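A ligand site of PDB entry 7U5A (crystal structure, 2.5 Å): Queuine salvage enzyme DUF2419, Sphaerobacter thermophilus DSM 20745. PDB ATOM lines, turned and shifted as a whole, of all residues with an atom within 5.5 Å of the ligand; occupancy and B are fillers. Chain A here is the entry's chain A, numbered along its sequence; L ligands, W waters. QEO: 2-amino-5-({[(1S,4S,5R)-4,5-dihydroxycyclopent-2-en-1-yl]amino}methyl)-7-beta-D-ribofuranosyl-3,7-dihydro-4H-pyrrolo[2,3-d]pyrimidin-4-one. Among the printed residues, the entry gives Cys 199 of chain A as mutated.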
ATOM      1  N   PRO A  46      13.204  20.456  -9.279  1.00  0.00           N
ATOM      2  CA  PRO A  46      14.481  19.751  -9.279  1.00  0.00           C
ATOM      3  C   PRO A  46      14.197  18.260  -9.124  1.00  0.00           C
ATOM      4  O   PRO A  46      13.125  17.904  -8.653  1.00  0.00           O
ATOM      5  CB  PRO A  46      15.258  20.300  -8.079  1.00  0.00           C
ATOM      6  CG  PRO A  46      14.559  21.616  -7.757  1.00  0.00           C
ATOM      7  CD  PRO A  46      13.114  21.453  -8.199  1.00  0.00           C
ATOM      8  N   THR A  47      15.136  17.399  -9.519  1.00  0.00           N
ATOM      9  CA  THR A  47      14.968  15.943  -9.356  1.00  0.00           C
ATOM     10  C   THR A  47      15.195  15.648  -7.874  1.00  0.00           C
ATOM     11  O   THR A  47      14.281  15.950  -7.083  1.00  0.00           O
ATOM     12  CB  THR A  47      15.901  15.192 -10.314  1.00  0.00           C
ATOM     13  OG1 THR A  47      17.227  15.704 -10.096  1.00  0.00           O
ATOM     14  CG2 THR A  47      15.516  15.380 -11.760  1.00  0.00           C
ATOM     15  N   TRP A  48      16.362  15.125  -7.522  1.00  0.00           N
ATOM     16  CA  TRP A  48      16.792  14.982  -6.100  1.00  0.00           C
ATOM     17  C   TRP A  48      18.318  15.048  -6.071  1.00  0.00           C
ATOM     18  O   TRP A  48      18.978  14.126  -6.604  1.00  0.00           O
ATOM     19  CB  TRP A  48      16.247  13.693  -5.481  1.00  0.00           C
ATOM     20  CG  TRP A  48      16.343  13.665  -3.988  1.00  0.00           C
ATOM     21  CD1 TRP A  48      15.504  14.257  -3.084  1.00  0.00           C
ATOM     22  CD2 TRP A  48      17.347  12.995  -3.208  1.00  0.00           C
ATOM     23  NE1 TRP A  48      15.918  14.017  -1.800  1.00  0.00           N
ATOM     24  CE2 TRP A  48      17.048  13.240  -1.844  1.00  0.00           C
ATOM     25  CE3 TRP A  48      18.473  12.223  -3.527  1.00  0.00           C
ATOM     26  CZ2 TRP A  48      17.830  12.738  -0.817  1.00  0.00           C
ATOM     27  CZ3 TRP A  48      19.244  11.721  -2.508  1.00  0.00           C
ATOM     28  CH2 TRP A  48      18.927  11.978  -1.167  1.00  0.00           C
ATOM     29  N   ASN A  49      18.842  16.135  -5.494  1.00  0.00           N
ATOM     30  CA  ASN A  49      20.267  16.542  -5.650  1.00  0.00           C
ATOM     31  C   ASN A  49      21.156  15.502  -4.947  1.00  0.00           C
ATOM     32  O   ASN A  49      21.580  15.741  -3.791  1.00  0.00           O
ATOM     33  CB  ASN A  49      20.462  17.984  -5.175  1.00  0.00           C
ATOM     34  CG  ASN A  49      21.177  18.856  -6.199  1.00  0.00           C
ATOM     35  OD1 ASN A  49      21.986  18.361  -6.986  1.00  0.00           O
ATOM     36  ND2 ASN A  49      20.874  20.144  -6.196  1.00  0.00           N
ATOM     37  N   ASN A  72      17.214  18.647  10.537  1.00  0.00           N
ATOM     38  CA  ASN A  72      16.974  19.572   9.402  1.00  0.00           C
ATOM     39  C   ASN A  72      16.124  20.759   9.866  1.00  0.00           C
ATOM     40  O   ASN A  72      14.891  20.737   9.669  1.00  0.00           O
ATOM     41  CB  ASN A  72      16.287  18.865   8.234  1.00  0.00           C
ATOM     42  CG  ASN A  72      15.997  19.803   7.074  1.00  0.00           C
ATOM     43  OD1 ASN A  72      16.411  20.962   7.088  1.00  0.00           O
ATOM     44  ND2 ASN A  72      15.281  19.307   6.079  1.00  0.00           N
ATOM     45  N   PHE A  73      16.767  21.793  10.433  1.00  0.00           N
ATOM     46  CA  PHE A  73      16.089  22.996  10.958  1.00  0.00           C
ATOM     47  C   PHE A  73      17.104  24.101  11.286  1.00  0.00           C
ATOM     48  O   PHE A  73      18.285  23.807  11.504  1.00  0.00           O
ATOM     49  CB  PHE A  73      15.259  22.659  12.198  1.00  0.00           C
ATOM     50  CG  PHE A  73      16.025  22.067  13.358  1.00  0.00           C
ATOM     51  CD1 PHE A  73      16.752  22.877  14.223  1.00  0.00           C
ATOM     52  CD2 PHE A  73      15.999  20.707  13.616  1.00  0.00           C
ATOM     53  CE1 PHE A  73      17.443  22.345  15.299  1.00  0.00           C
ATOM     54  CE2 PHE A  73      16.683  20.166  14.701  1.00  0.00           C
ATOM     55  CZ  PHE A  73      17.405  20.984  15.536  1.00  0.00           C
ATOM     56  N   CYS A  74      16.613  25.342  11.263  1.00  0.00           N
ATOM     57  CA  CYS A  74      17.209  26.573  11.854  1.00  0.00           C
ATOM     58  C   CYS A  74      18.728  26.683  11.621  1.00  0.00           C
ATOM     59  O   CYS A  74      19.521  26.256  12.495  1.00  0.00           O
ATOM     60  CB  CYS A  74      16.889  26.632  13.343  1.00  0.00           C
ATOM     61  SG  CYS A  74      17.209  28.269  14.054  1.00  0.00           S
ATOM     62  N   PHE A  75      19.122  27.314  10.509  1.00  0.00           N
ATOM     63  CA  PHE A  75      20.526  27.392  10.051  1.00  0.00           C
ATOM     64  C   PHE A  75      21.044  28.833  10.116  1.00  0.00           C
ATOM     65  O   PHE A  75      22.175  29.075   9.654  1.00  0.00           O
ATOM     66  CB  PHE A  75      20.654  26.864   8.622  1.00  0.00           C
ATOM     67  CG  PHE A  75      20.182  25.445   8.459  1.00  0.00           C
ATOM     68  CD1 PHE A  75      20.828  24.411   9.126  1.00  0.00           C
ATOM     69  CD2 PHE A  75      19.101  25.137   7.650  1.00  0.00           C
ATOM     70  CE1 PHE A  75      20.393  23.094   9.000  1.00  0.00           C
ATOM     71  CE2 PHE A  75      18.676  23.824   7.523  1.00  0.00           C
ATOM     72  CZ  PHE A  75      19.316  22.802   8.187  1.00  0.00           C
ATOM     73  N   TYR A  93      20.957  24.540   4.523  1.00  0.00           N
ATOM     74  CA  TYR A  93      20.595  23.103   4.421  1.00  0.00           C
ATOM     75  C   TYR A  93      21.716  22.342   3.711  1.00  0.00           C
ATOM     76  O   TYR A  93      21.985  21.191   4.106  1.00  0.00           O
ATOM     77  CB  TYR A  93      19.257  22.937   3.699  1.00  0.00           C
ATOM     78  CG  TYR A  93      18.933  21.531   3.287  1.00  0.00           C
ATOM     79  CD1 TYR A  93      18.375  20.623   4.189  1.00  0.00           C
ATOM     80  CD2 TYR A  93      19.151  21.101   1.997  1.00  0.00           C
ATOM     81  CE1 TYR A  93      18.058  19.334   3.797  1.00  0.00           C
ATOM     82  CE2 TYR A  93      18.847  19.808   1.599  1.00  0.00           C
ATOM     83  CZ  TYR A  93      18.293  18.917   2.497  1.00  0.00           C
ATOM     84  OH  TYR A  93      17.984  17.658   2.084  1.00  0.00           O
ATOM     85  N   TRP A  94      22.355  22.925   2.695  1.00  0.00           N
ATOM     86  CA  TRP A  94      23.417  22.212   1.924  1.00  0.00           C
ATOM     87  C   TRP A  94      24.644  21.971   2.803  1.00  0.00           C
ATOM     88  O   TRP A  94      25.271  20.914   2.637  1.00  0.00           O
ATOM     89  CB  TRP A  94      23.736  22.931   0.599  1.00  0.00           C
ATOM     90  CG  TRP A  94      22.628  22.808  -0.392  1.00  0.00           C
ATOM     91  CD1 TRP A  94      22.018  23.836  -1.051  1.00  0.00           C
ATOM     92  CD2 TRP A  94      21.968  21.606  -0.823  1.00  0.00           C
ATOM     93  NE1 TRP A  94      21.029  23.352  -1.875  1.00  0.00           N
ATOM     94  CE2 TRP A  94      20.974  21.982  -1.759  1.00  0.00           C
ATOM     95  CE3 TRP A  94      22.120  20.244  -0.529  1.00  0.00           C
ATOM     96  CZ2 TRP A  94      20.152  21.055  -2.384  1.00  0.00           C
ATOM     97  CZ3 TRP A  94      21.296  19.325  -1.148  1.00  0.00           C
ATOM     98  CH2 TRP A  94      20.321  19.736  -2.069  1.00  0.00           C
ATOM     99  N   CYS A 199       6.100  19.406   9.430  1.00  0.00           N
ATOM    100  CA  CYS A 199       7.099  19.884   8.450  1.00  0.00           C
ATOM    101  C   CYS A 199       8.173  18.816   8.250  1.00  0.00           C
ATOM    102  O   CYS A 199       8.166  18.165   7.193  1.00  0.00           O
ATOM    103  CB  CYS A 199       7.679  21.211   8.935  1.00  0.00           C
ATOM    104  SG  CYS A 199       8.911  21.883   7.800  1.00  0.00           S
ATOM    105  N   ARG A 200       9.037  18.584   9.243  1.00  0.00           N
ATOM    106  CA  ARG A 200      10.197  17.659   9.100  1.00  0.00           C
ATOM    107  C   ARG A 200       9.699  16.234   8.844  1.00  0.00           C
ATOM    108  O   ARG A 200      10.356  15.508   8.091  1.00  0.00           O
ATOM    109  CB  ARG A 200      11.117  17.732  10.319  1.00  0.00           C
ATOM    110  CG  ARG A 200      11.896  19.046  10.402  1.00  0.00           C
ATOM    111  CD  ARG A 200      12.948  19.085  11.483  1.00  0.00           C
ATOM    112  NE  ARG A 200      12.364  19.014  12.812  1.00  0.00           N
ATOM    113  CZ  ARG A 200      12.478  17.989  13.650  1.00  0.00           C
ATOM    114  NH1 ARG A 200      13.168  16.903  13.324  1.00  0.00           N
ATOM    115  NH2 ARG A 200      11.888  18.033  14.833  1.00  0.00           N
ATOM    116  N   ILE A 203       8.559  16.129   5.034  1.00  0.00           N
ATOM    117  CA  ILE A 203       9.695  16.256   4.076  1.00  0.00           C
ATOM    118  C   ILE A 203      10.457  14.923   4.038  1.00  0.00           C
ATOM    119  O   ILE A 203      10.802  14.460   2.928  1.00  0.00           O
ATOM    120  CB  ILE A 203      10.588  17.473   4.402  1.00  0.00           C
ATOM    121  CG1 ILE A 203      11.383  17.922   3.169  1.00  0.00           C
ATOM    122  CG2 ILE A 203      11.507  17.226   5.586  1.00  0.00           C
ATOM    123  CD1 ILE A 203      11.960  19.315   3.294  1.00  0.00           C
ATOM    124  N   ASP A 207      11.887  12.877   0.884  1.00  0.00           N
ATOM    125  CA  ASP A 207      13.353  12.627   0.718  1.00  0.00           C
ATOM    126  C   ASP A 207      13.571  11.137   0.403  1.00  0.00           C
ATOM    127  O   ASP A 207      14.405  10.850  -0.484  1.00  0.00           O
ATOM    128  CB  ASP A 207      14.153  13.146   1.917  1.00  0.00           C
ATOM    129  CG  ASP A 207      14.443  14.653   1.903  1.00  0.00           C
ATOM    130  OD1 ASP A 207      14.210  15.316   0.851  1.00  0.00           O
ATOM    131  OD2 ASP A 207      14.897  15.166   2.960  1.00  0.00           O
ATOM    132  N   PHE A 229       6.047  21.944   3.133  1.00  0.00           N
ATOM    133  CA  PHE A 229       6.856  21.815   4.365  1.00  0.00           C
ATOM    134  C   PHE A 229       7.068  23.228   4.890  1.00  0.00           C
ATOM    135  O   PHE A 229       7.973  23.932   4.405  1.00  0.00           O
ATOM    136  CB  PHE A 229       8.142  21.046   4.031  1.00  0.00           C
ATOM    137  CG  PHE A 229       7.942  19.907   3.059  1.00  0.00           C
ATOM    138  CD1 PHE A 229       7.008  18.909   3.316  1.00  0.00           C
ATOM    139  CD2 PHE A 229       8.667  19.850   1.872  1.00  0.00           C
ATOM    140  CE1 PHE A 229       6.815  17.874   2.417  1.00  0.00           C
ATOM    141  CE2 PHE A 229       8.468  18.806   0.983  1.00  0.00           C
ATOM    142  CZ  PHE A 229       7.552  17.818   1.251  1.00  0.00           C
ATOM    143  N   ALA A 230       6.212  23.651   5.807  1.00  0.00           N
ATOM    144  CA  ALA A 230       6.122  25.051   6.292  1.00  0.00           C
ATOM    145  C   ALA A 230       7.332  25.355   7.189  1.00  0.00           C
ATOM    146  O   ALA A 230       7.214  25.128   8.390  1.00  0.00           O
ATOM    147  CB  ALA A 230       4.819  25.260   7.022  1.00  0.00           C
ATOM    148  N   ASP A 231       8.438  25.845   6.618  1.00  0.00           N
ATOM    149  CA  ASP A 231       9.535  26.476   7.397  1.00  0.00           C
ATOM    150  C   ASP A 231       9.666  27.936   6.945  1.00  0.00           C
ATOM    151  O   ASP A 231       8.605  28.590   6.819  1.00  0.00           O
ATOM    152  CB  ASP A 231      10.826  25.654   7.370  1.00  0.00           C
ATOM    153  CG  ASP A 231      11.736  25.906   8.566  1.00  0.00           C
ATOM    154  OD1 ASP A 231      11.297  26.636   9.492  1.00  0.00           O
ATOM    155  OD2 ASP A 231      12.875  25.379   8.573  1.00  0.00           O
ATOM    156  N   TYR A 232      10.876  28.456   6.722  1.00  0.00           N
ATOM    157  CA  TYR A 232      11.071  29.920   6.544  1.00  0.00           C
ATOM    158  C   TYR A 232      11.460  30.285   5.104  1.00  0.00           C
ATOM    159  O   TYR A 232      11.249  31.462   4.754  1.00  0.00           O
ATOM    160  CB  TYR A 232      12.038  30.501   7.579  1.00  0.00           C
ATOM    161  CG  TYR A 232      13.449  29.955   7.617  1.00  0.00           C
ATOM    162  CD1 TYR A 232      14.385  30.299   6.651  1.00  0.00           C
ATOM    163  CD2 TYR A 232      13.859  29.146   8.657  1.00  0.00           C
ATOM    164  CE1 TYR A 232      15.686  29.813   6.713  1.00  0.00           C
ATOM    165  CE2 TYR A 232      15.151  28.659   8.734  1.00  0.00           C
ATOM    166  CZ  TYR A 232      16.069  28.994   7.755  1.00  0.00           C
ATOM    167  OH  TYR A 232      17.349  28.511   7.839  1.00  0.00           O
ATOM    168  N   LYS A 233      11.959  29.351   4.278  1.00  0.00           N
ATOM    169  CA  LYS A 233      12.390  29.732   2.907  1.00  0.00           C
ATOM    170  C   LYS A 233      11.169  29.901   2.007  1.00  0.00           C
ATOM    171  O   LYS A 233      11.106  30.914   1.315  1.00  0.00           O
ATOM    172  CB  LYS A 233      13.367  28.731   2.282  1.00  0.00           C
ATOM    173  CG  LYS A 233      14.837  28.944   2.612  1.00  0.00           C
ATOM    174  CD  LYS A 233      15.353  30.375   2.476  1.00  0.00           C
ATOM    175  CE  LYS A 233      15.427  30.875   1.053  1.00  0.00           C
ATOM    176  NZ  LYS A 233      16.161  32.157   0.962  1.00  0.00           N
ATOM    177  N   VAL A 234      10.239  28.946   2.009  1.00  0.00           N
ATOM    178  CA  VAL A 234       9.109  28.936   1.044  1.00  0.00           C
ATOM    179  C   VAL A 234       8.245  30.178   1.230  1.00  0.00           C
ATOM    180  O   VAL A 234       7.936  30.830   0.245  1.00  0.00           O
ATOM    181  CB  VAL A 234       8.325  27.610   1.101  1.00  0.00           C
ATOM    182  CG1 VAL A 234       7.063  27.656   0.263  1.00  0.00           C
ATOM    183  CG2 VAL A 234       9.210  26.449   0.653  1.00  0.00           C
ATOM    184  N   ASP A 298       6.264  22.896  -3.711  1.00  0.00           N
ATOM    185  CA  ASP A 298       7.124  23.311  -2.570  1.00  0.00           C
ATOM    186  C   ASP A 298       8.606  23.184  -2.971  1.00  0.00           C
ATOM    187  O   ASP A 298       9.380  24.125  -2.710  1.00  0.00           O
ATOM    188  CB  ASP A 298       6.770  22.534  -1.305  1.00  0.00           C
ATOM    189  CG  ASP A 298       7.788  22.690  -0.190  1.00  0.00           C
ATOM    190  OD1 ASP A 298       8.911  22.218  -0.376  1.00  0.00           O
ATOM    191  OD2 ASP A 298       7.443  23.293   0.834  1.00  0.00           O
ATOM    192  N   TRP A 299       8.971  22.044  -3.560  1.00  0.00           N
ATOM    193  CA  TRP A 299      10.355  21.722  -4.022  1.00  0.00           C
ATOM    194  C   TRP A 299      10.827  22.796  -5.001  1.00  0.00           C
ATOM    195  O   TRP A 299      11.980  23.254  -4.915  1.00  0.00           O
ATOM    196  CB  TRP A 299      10.390  20.340  -4.683  1.00  0.00           C
ATOM    197  CG  TRP A 299      10.618  19.188  -3.754  1.00  0.00           C
ATOM    198  CD1 TRP A 299      10.547  19.195  -2.391  1.00  0.00           C
ATOM    199  CD2 TRP A 299      10.924  17.840  -4.134  1.00  0.00           C
ATOM    200  NE1 TRP A 299      10.811  17.945  -1.896  1.00  0.00           N
ATOM    201  CE2 TRP A 299      11.040  17.091  -2.948  1.00  0.00           C
ATOM    202  CE3 TRP A 299      11.115  17.200  -5.360  1.00  0.00           C
ATOM    203  CZ2 TRP A 299      11.339  15.730  -2.957  1.00  0.00           C
ATOM    204  CZ3 TRP A 299      11.411  15.847  -5.363  1.00  0.00           C
ATOM    205  CH2 TRP A 299      11.526  15.131  -4.170  1.00  0.00           C
ATOM    206  N   TRP A 302      11.140  26.251  -2.975  1.00  0.00           N
ATOM    207  CA  TRP A 302      12.387  26.206  -2.180  1.00  0.00           C
ATOM    208  C   TRP A 302      13.579  26.385  -3.113  1.00  0.00           C
ATOM    209  O   TRP A 302      14.555  27.069  -2.734  1.00  0.00           O
ATOM    210  CB  TRP A 302      12.505  24.904  -1.364  1.00  0.00           C
ATOM    211  CG  TRP A 302      13.612  24.952  -0.357  1.00  0.00           C
ATOM    212  CD1 TRP A 302      13.522  25.338   0.950  1.00  0.00           C
ATOM    213  CD2 TRP A 302      14.996  24.602  -0.567  1.00  0.00           C
ATOM    214  NE1 TRP A 302      14.741  25.244   1.568  1.00  0.00           N
ATOM    215  CE2 TRP A 302      15.662  24.793   0.649  1.00  0.00           C
ATOM    216  CE3 TRP A 302      15.722  24.139  -1.671  1.00  0.00           C
ATOM    217  CZ2 TRP A 302      17.026  24.542   0.808  1.00  0.00           C
ATOM    218  CZ3 TRP A 302      17.069  23.902  -1.522  1.00  0.00           C
ATOM    219  CH2 TRP A 302      17.713  24.093  -0.299  1.00  0.00           C
ATOM    220  N   ASP A 303      13.491  25.795  -4.312  1.00  0.00           N
ATOM    221  CA  ASP A 303      14.526  25.882  -5.370  1.00  0.00           C
ATOM    222  C   ASP A 303      14.751  27.369  -5.727  1.00  0.00           C
ATOM    223  O   ASP A 303      15.919  27.812  -5.667  1.00  0.00           O
ATOM    224  CB  ASP A 303      14.140  25.017  -6.564  1.00  0.00           C
ATOM    225  CG  ASP A 303      15.202  24.953  -7.649  1.00  0.00           C
ATOM    226  OD1 ASP A 303      16.358  24.643  -7.298  1.00  0.00           O
ATOM    227  OD2 ASP A 303      14.858  25.226  -8.838  1.00  0.00           O
HETATM  228  O5' QEO L   1      11.623  23.457   5.222  1.00  0.00           O
HETATM  229  C5' QEO L   1      12.035  22.435   6.132  1.00  0.00           C
HETATM  230  C4' QEO L   1      13.533  22.356   6.277  1.00  0.00           C
HETATM  231  C3' QEO L   1      14.295  23.697   6.297  1.00  0.00           C
HETATM  232  O3' QEO L   1      15.386  23.607   7.202  1.00  0.00           O
HETATM  233  C2' QEO L   1      14.782  23.877   4.859  1.00  0.00           C
HETATM  234  O2' QEO L   1      15.990  24.617   4.792  1.00  0.00           O
HETATM  235  O4' QEO L   1      14.076  21.623   5.157  1.00  0.00           O
HETATM  236  C1' QEO L   1      14.984  22.424   4.414  1.00  0.00           C
HETATM  237  N2  QEO L   1      14.698  22.118   3.026  1.00  0.00           N
HETATM  238  C10 QEO L   1      13.497  22.271   2.389  1.00  0.00           C
HETATM  239  N3  QEO L   1      12.353  22.809   2.900  1.00  0.00           N
HETATM  240  C12 QEO L   1      11.311  22.846   2.056  1.00  0.00           C
HETATM  241  N5  QEO L   1      10.137  23.355   2.450  1.00  0.00           N
HETATM  242  N4  QEO L   1      11.378  22.390   0.763  1.00  0.00           N
HETATM  243  C11 QEO L   1      12.526  21.828   0.200  1.00  0.00           C
HETATM  244  O3  QEO L   1      12.508  21.444  -0.985  1.00  0.00           O
HETATM  245  C9  QEO L   1      13.643  21.776   1.083  1.00  0.00           C
HETATM  246  C8  QEO L   1      15.598  21.520   2.159  1.00  0.00           C
HETATM  247  C7  QEO L   1      14.997  21.305   0.955  1.00  0.00           C
HETATM  248  C6  QEO L   1      15.657  20.693  -0.241  1.00  0.00           C
HETATM  249  N1  QEO L   1      14.720  19.930  -1.044  1.00  0.00           N
HETATM  250  C1  QEO L   1      15.321  19.285  -2.204  1.00  0.00           C
HETATM  251  C2  QEO L   1      15.263  20.106  -3.499  1.00  0.00           C
HETATM  252  O1  QEO L   1      16.432  20.908  -3.599  1.00  0.00           O
HETATM  253  C3  QEO L   1      14.518  18.053  -2.556  1.00  0.00           C
HETATM  254  C5  QEO L   1      14.414  17.927  -3.873  1.00  0.00           C
HETATM  255  C4  QEO L   1      15.183  19.024  -4.561  1.00  0.00           C
HETATM  256  O2  QEO L   1      16.447  18.552  -4.999  1.00  0.00           O
HETATM  257  O   HOH W   1      16.047  25.842   8.316  1.00  0.00           O
HETATM  258  O   HOH W   2      12.805  22.889   9.597  1.00  0.00           O
HETATM  259  O   HOH W   3      12.087  26.093   4.312  1.00  0.00           O
HETATM  260  O   HOH W   4      14.606  26.815   5.656  1.00  0.00           O
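N2 of the ligand sits close to NE1 of Trp 302. CB of Pro 46 touches O2 of the ligand, 3.7 Å away. Thr 47 touches the ligand. Trp 48 touches the ligand. Phe 73 touches the ligand (CA to O3', 3.9 Å). Phe 75 touches the ligand. Tyr 93 touches the ligand (CG to C8, 3.5 Å). Trp 94 touches the ligand. SG of Cys 199 touches C5' of the ligand, at 3.6 Å. Ile 203 touches the ligand (CD1 to C10, 3.5 Å). CG2 of Val 234 touches N5 of the ligand, at 3.7 Å. Trp 299 touches the ligand (CD1 to O3, 3.3 Å). Hydrophobic or aromatic side chains that line the ligand: Pro 46, Trp 48, Phe 75, Tyr 93, Trp 94, Ile 203, Phe 229, Val 234, Trp 299 and Trp 302. The nearest printed residue that does not touch the ligand is Asp 207 (4.4 Å).
Water W1 lies within hydrogen-bond range of O3' of the ligand, OH of Tyr 232, N of Cys 74 and OD2 of Asp 231. Water W3 bridges O5' of the ligand (2.8 Å) and N of Lys 233 (3.3 Å). Water W2 lies within hydrogen-bond range of OD2 of Asp 231 (2.7 Å) and O of Asn 72 (3.0 Å).
OD1 of Asp 298 sits at hydrogen-bond distance from N4 of the ligand, 2.7 Å away. O4' of the ligand sits at hydrogen-bond distance from ND2 of Asn 72 (2.8 Å). N5 of the ligand lies within hydrogen-bond range of O of Phe 229. O3' of the ligand sits close to OD2 of Asp 231 (3.4 Å). N of Asn 49 sits at hydrogen-bond distance from O2 of the ligand (3.4 Å).
OD2 of Asp 298 is in hydrogen-bond range of N of Phe 229 (3.0 Å). The side-chain hydroxyl (OH) of Tyr 232 sits at hydrogen-bond distance from the backbone NH (N) of Phe 75 (3.4 Å). The side-chain sulfur of Cys 199 lies within hydrogen-bond range of the backbone carbonyl oxygen of Ala 230, at 3.7 Å. NE1 of Trp 48 is in hydrogen-bond range of OD1 of Asp 207, 3.4 Å away.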
